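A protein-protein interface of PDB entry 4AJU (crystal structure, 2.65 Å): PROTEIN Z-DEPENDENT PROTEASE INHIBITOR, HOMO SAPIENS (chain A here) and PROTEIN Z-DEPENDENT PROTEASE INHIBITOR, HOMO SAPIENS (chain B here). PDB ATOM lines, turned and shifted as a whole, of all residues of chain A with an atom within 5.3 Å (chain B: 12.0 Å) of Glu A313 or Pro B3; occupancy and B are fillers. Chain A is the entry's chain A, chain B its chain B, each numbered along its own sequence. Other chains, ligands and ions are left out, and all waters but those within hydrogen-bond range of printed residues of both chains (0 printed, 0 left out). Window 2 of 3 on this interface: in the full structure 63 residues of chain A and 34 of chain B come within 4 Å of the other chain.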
ATOM      1  N   TYR A 249       3.394  25.900  19.047  1.00  0.00           N
ATOM      2  CA  TYR A 249       4.245  25.555  17.901  1.00  0.00           C
ATOM      3  C   TYR A 249       5.637  25.123  18.313  1.00  0.00           C
ATOM      4  O   TYR A 249       6.319  25.844  19.029  1.00  0.00           O
ATOM      5  CB  TYR A 249       4.371  26.758  16.980  1.00  0.00           C
ATOM      6  CG  TYR A 249       5.271  26.545  15.793  1.00  0.00           C
ATOM      7  CD1 TYR A 249       4.817  25.874  14.663  1.00  0.00           C
ATOM      8  CD2 TYR A 249       6.576  27.026  15.785  1.00  0.00           C
ATOM      9  CE1 TYR A 249       5.636  25.689  13.554  1.00  0.00           C
ATOM     10  CE2 TYR A 249       7.405  26.845  14.677  1.00  0.00           C
ATOM     11  CZ  TYR A 249       6.927  26.174  13.568  1.00  0.00           C
ATOM     12  OH  TYR A 249       7.746  25.982  12.475  1.00  0.00           O
ATOM     13  N   GLY A 250       6.066  23.958  17.845  1.00  0.00           N
ATOM     14  CA  GLY A 250       7.444  23.523  18.033  1.00  0.00           C
ATOM     15  C   GLY A 250       8.063  23.015  16.751  1.00  0.00           C
ATOM     16  O   GLY A 250       7.380  22.424  15.922  1.00  0.00           O
ATOM     17  N   ALA A 251       9.363  23.234  16.588  1.00  0.00           N
ATOM     18  CA  ALA A 251      10.085  22.766  15.405  1.00  0.00           C
ATOM     19  C   ALA A 251      11.321  22.034  15.872  1.00  0.00           C
ATOM     20  O   ALA A 251      12.161  22.610  16.536  1.00  0.00           O
ATOM     21  CB  ALA A 251      10.470  23.937  14.502  1.00  0.00           C
ATOM     22  N   GLY A 252      11.427  20.757  15.547  1.00  0.00           N
ATOM     23  CA  GLY A 252      12.622  20.010  15.864  1.00  0.00           C
ATOM     24  C   GLY A 252      12.406  18.540  15.636  1.00  0.00           C
ATOM     25  O   GLY A 252      11.517  18.145  14.883  1.00  0.00           O
ATOM     26  N   ASN A 311      13.398  15.752  11.786  1.00  0.00           N
ATOM     27  CA  ASN A 311      13.108  17.172  11.970  1.00  0.00           C
ATOM     28  C   ASN A 311      11.749  17.434  11.356  1.00  0.00           C
ATOM     29  O   ASN A 311      11.513  17.088  10.193  1.00  0.00           O
ATOM     30  CB  ASN A 311      14.155  18.075  11.289  1.00  0.00           C
ATOM     31  CG  ASN A 311      15.409  18.281  12.139  1.00  0.00           C
ATOM     32  OD1 ASN A 311      15.337  18.399  13.368  1.00  0.00           O
ATOM     33  ND2 ASN A 311      16.564  18.340  11.482  1.00  0.00           N
ATOM     34  N   MET A 312      10.852  18.021  12.137  1.00  0.00           N
ATOM     35  CA  MET A 312       9.538  18.379  11.624  1.00  0.00           C
ATOM     36  C   MET A 312       8.900  19.491  12.438  1.00  0.00           C
ATOM     37  O   MET A 312       9.375  19.825  13.519  1.00  0.00           O
ATOM     38  CB  MET A 312       8.630  17.148  11.596  1.00  0.00           C
ATOM     39  CG  MET A 312       8.378  16.539  12.938  1.00  0.00           C
ATOM     40  SD  MET A 312       7.518  14.974  12.784  1.00  0.00           S
ATOM     41  CE  MET A 312       5.925  15.512  12.159  1.00  0.00           C
ATOM     42  N   GLU A 313       7.820  20.054  11.908  1.00  0.00           N
ATOM     43  CA  GLU A 313       7.110  21.142  12.570  1.00  0.00           C
ATOM     44  C   GLU A 313       5.791  20.630  13.116  1.00  0.00           C
ATOM     45  O   GLU A 313       5.083  19.900  12.430  1.00  0.00           O
ATOM     46  CB  GLU A 313       6.871  22.289  11.600  1.00  0.00           C
ATOM     47  CG  GLU A 313       8.140  22.769  10.923  1.00  0.00           C
ATOM     48  CD  GLU A 313       7.906  23.940  10.018  1.00  0.00           C
ATOM     49  OE1 GLU A 313       6.742  24.380   9.880  1.00  0.00           O
ATOM     50  OE2 GLU A 313       8.892  24.429   9.432  1.00  0.00           O
ATOM     51  N   VAL A 314       5.481  21.008  14.354  1.00  0.00           N
ATOM     52  CA  VAL A 314       4.304  20.518  15.050  1.00  0.00           C
ATOM     53  C   VAL A 314       3.456  21.677  15.545  1.00  0.00           C
ATOM     54  O   VAL A 314       3.950  22.544  16.271  1.00  0.00           O
ATOM     55  CB  VAL A 314       4.694  19.661  16.273  1.00  0.00           C
ATOM     56  CG1 VAL A 314       3.457  19.326  17.113  1.00  0.00           C
ATOM     57  CG2 VAL A 314       5.431  18.391  15.837  1.00  0.00           C
ATOM     58  N   PHE A 315       2.185  21.693  15.142  1.00  0.00           N
ATOM     59  CA  PHE A 315       1.195  22.586  15.734  1.00  0.00           C
ATOM     60  C   PHE A 315       0.271  21.767  16.611  1.00  0.00           C
ATOM     61  O   PHE A 315      -0.278  20.764  16.159  1.00  0.00           O
ATOM     62  CB  PHE A 315       0.361  23.273  14.666  1.00  0.00           C
ATOM     63  CG  PHE A 315       1.126  24.234  13.803  1.00  0.00           C
ATOM     64  CD1 PHE A 315       1.871  23.782  12.729  1.00  0.00           C
ATOM     65  CD2 PHE A 315       1.061  25.596  14.036  1.00  0.00           C
ATOM     66  CE1 PHE A 315       2.553  24.667  11.911  1.00  0.00           C
ATOM     67  CE2 PHE A 315       1.738  26.489  13.214  1.00  0.00           C
ATOM     68  CZ  PHE A 315       2.488  26.019  12.155  1.00  0.00           C
ATOM     69  N   SER B   1      13.894  18.540   1.339  1.00  0.00           N
ATOM     70  CA  SER B   1      14.300  19.975   1.424  1.00  0.00           C
ATOM     71  C   SER B   1      13.159  20.873   1.927  1.00  0.00           C
ATOM     72  O   SER B   1      13.189  22.094   1.725  1.00  0.00           O
ATOM     73  CB  SER B   1      14.790  20.465   0.060  1.00  0.00           C
ATOM     74  OG  SER B   1      15.367  21.758   0.152  1.00  0.00           O
ATOM     75  N   MET B   2      12.161  20.267   2.572  1.00  0.00           N
ATOM     76  CA  MET B   2      11.055  21.017   3.174  1.00  0.00           C
ATOM     77  C   MET B   2      10.428  20.180   4.299  1.00  0.00           C
ATOM     78  O   MET B   2       9.709  19.219   4.026  1.00  0.00           O
ATOM     79  CB  MET B   2      10.005  21.384   2.110  1.00  0.00           C
ATOM     80  CG  MET B   2       9.089  22.550   2.515  1.00  0.00           C
ATOM     81  SD  MET B   2       9.767  24.186   2.122  1.00  0.00           S
ATOM     82  CE  MET B   2       9.172  25.161   3.511  1.00  0.00           C
ATOM     83  N   PRO B   3      10.698  20.540   5.568  1.00  0.00           N
ATOM     84  CA  PRO B   3      10.337  19.643   6.682  1.00  0.00           C
ATOM     85  C   PRO B   3       8.848  19.279   6.732  1.00  0.00           C
ATOM     86  O   PRO B   3       8.006  20.094   6.364  1.00  0.00           O
ATOM     87  CB  PRO B   3      10.743  20.443   7.930  1.00  0.00           C
ATOM     88  CG  PRO B   3      10.806  21.866   7.478  1.00  0.00           C
ATOM     89  CD  PRO B   3      11.252  21.819   6.050  1.00  0.00           C
ATOM     90  N   PRO B   4       8.522  18.054   7.168  1.00  0.00           N
ATOM     91  CA  PRO B   4       7.109  17.715   7.328  1.00  0.00           C
ATOM     92  C   PRO B   4       6.446  18.594   8.374  1.00  0.00           C
ATOM     93  O   PRO B   4       7.124  19.077   9.271  1.00  0.00           O
ATOM     94  CB  PRO B   4       7.144  16.257   7.802  1.00  0.00           C
ATOM     95  CG  PRO B   4       8.464  15.741   7.342  1.00  0.00           C
ATOM     96  CD  PRO B   4       9.397  16.900   7.433  1.00  0.00           C
ATOM     97  N   VAL B   5       5.141  18.813   8.242  1.00  0.00           N
ATOM     98  CA  VAL B   5       4.373  19.567   9.225  1.00  0.00           C
ATOM     99  C   VAL B   5       3.190  18.728   9.655  1.00  0.00           C
ATOM    100  O   VAL B   5       2.426  18.288   8.806  1.00  0.00           O
ATOM    101  CB  VAL B   5       3.831  20.889   8.649  1.00  0.00           C
ATOM    102  CG1 VAL B   5       2.975  21.602   9.688  1.00  0.00           C
ATOM    103  CG2 VAL B   5       4.973  21.787   8.183  1.00  0.00           C
ATOM    104  N   ILE B   6       3.056  18.490  10.958  1.00  0.00           N
ATOM    105  CA  ILE B   6       1.864  17.868  11.518  1.00  0.00           C
ATOM    106  C   ILE B   6       1.071  18.925  12.258  1.00  0.00           C
ATOM    107  O   ILE B   6       1.573  19.520  13.211  1.00  0.00           O
ATOM    108  CB  ILE B   6       2.192  16.760  12.526  1.00  0.00           C
ATOM    109  CG1 ILE B   6       2.543  15.463  11.811  1.00  0.00           C
ATOM    110  CG2 ILE B   6       1.011  16.498  13.418  1.00  0.00           C
ATOM    111  CD1 ILE B   6       2.883  14.324  12.768  1.00  0.00           C
ATOM    112  N   LYS B   7      -0.176  19.132  11.834  1.00  0.00           N
ATOM    113  CA  LYS B   7      -1.046  20.135  12.420  1.00  0.00           C
ATOM    114  C   LYS B   7      -2.263  19.451  13.038  1.00  0.00           C
ATOM    115  O   LYS B   7      -3.117  18.939  12.317  1.00  0.00           O
ATOM    116  CB  LYS B   7      -1.481  21.123  11.338  1.00  0.00           C
ATOM    117  CG  LYS B   7      -1.612  22.546  11.816  1.00  0.00           C
ATOM    118  CD  LYS B   7      -2.217  23.463  10.765  1.00  0.00           C
ATOM    119  CE  LYS B   7      -2.322  24.871  11.327  1.00  0.00           C
ATOM    120  NZ  LYS B   7      -3.183  25.748  10.507  1.00  0.00           N
ATOM    121  N   ILE B   8      -2.339  19.439  14.369  1.00  0.00           N
ATOM    122  CA  ILE B   8      -3.476  18.856  15.071  1.00  0.00           C
ATOM    123  C   ILE B   8      -4.600  19.873  15.022  1.00  0.00           C
ATOM    124  O   ILE B   8      -4.856  20.585  15.988  1.00  0.00           O
ATOM    125  CB  ILE B   8      -3.132  18.471  16.545  1.00  0.00           C
ATOM    126  CG1 ILE B   8      -2.163  17.295  16.584  1.00  0.00           C
ATOM    127  CG2 ILE B   8      -4.372  18.036  17.313  1.00  0.00           C
ATOM    128  CD1 ILE B   8      -0.807  17.594  16.028  1.00  0.00           C
ATOM    129  N   ASP B   9      -5.257  19.943  13.871  1.00  0.00           N
ATOM    130  CA  ASP B   9      -6.292  20.940  13.630  1.00  0.00           C
ATOM    131  C   ASP B   9      -7.638  20.259  13.429  1.00  0.00           C
ATOM    132  O   ASP B   9      -8.498  20.770  12.710  1.00  0.00           O
ATOM    133  CB  ASP B   9      -5.919  21.834  12.432  1.00  0.00           C
ATOM    134  CG  ASP B   9      -5.897  21.084  11.092  1.00  0.00           C
ATOM    135  OD1 ASP B   9      -5.731  19.842  11.078  1.00  0.00           O
ATOM    136  OD2 ASP B   9      -6.044  21.753  10.039  1.00  0.00           O
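Gly A250 touches none of the printed residues of chain B.
No residue of chain B comes within 4 Å of Gly A252.
Glu A313 touches just these residues of chain B: Pro B3, Pro B4, Val B5 and Ile B6.
Of the printed residues of chain A, Pro B3 touches Glu A313 (3.7 Å).
Printed residues of chain A within 4 Å of Pro B4: Asn A311, Met A312 and Glu A313.
Of the printed residues of chain A, Val B5 touches Glu A313 (3.3 Å) and Phe A315 (3.8 Å).
Of the printed residues of chain A, Ile B8 touches Phe A315 (3.0 Å).
The nearest residue of chain B that does not touch Glu A313 is Lys B7 (5.3 Å).
The nearest printed residue of chain A that does not touch Val B5 is Met A312 (4.9 Å).
Among the printed residues, merely in contact across the chains: Glu A313 with Val B5 (3.3 Å), Met A312 with Ile B6 (3.3 Å), Met A312 with Pro B4 (3.4 Å), Val A314 with Ile B6 (3.4 Å), Asn A311 with Pro B4 (3.5 Å), Phe A315 with Lys B7 (3.5 Å), Glu A313 with Pro B3 (3.7 Å) and Phe A315 with Val B5 (3.8 Å).
The backbone carbonyl oxygen (O) of Pro B4 sits at hydrogen-bond distance from the backbone NH (N) of Glu A313, at 2.9 Å.
The backbone carbonyl oxygen (O) of Glu A313 is in hydrogen-bond range of the backbone NH (N) of Ile B6, 2.9 Å away.
N of Phe A315 is in hydrogen-bond range of O of Ile B6 (3.0 Å).
The backbone carbonyl oxygen (O) of Phe A315 sits at hydrogen-bond distance from the backbone NH (N) of Ile B8 (3.0 Å).
Of the 9 printed residues of chain B, 6 touch a printed residue of chain A.
Among the printed residues, 12 pairs touch across the chains.
Among the printed residues, no Asp or Glu carboxylate lies within 4 Å of a Lys or Arg side-chain nitrogen of the other chain.
OE1 of Glu A313 lies close to OH of Tyr A249 (3.2 Å).
O of Gly A250 lies within hydrogen-bond range of N of Val A314, 2.8 Å away.
N of Met A312 is in hydrogen-bond range of O of Gly A252, at 2.8 Å.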
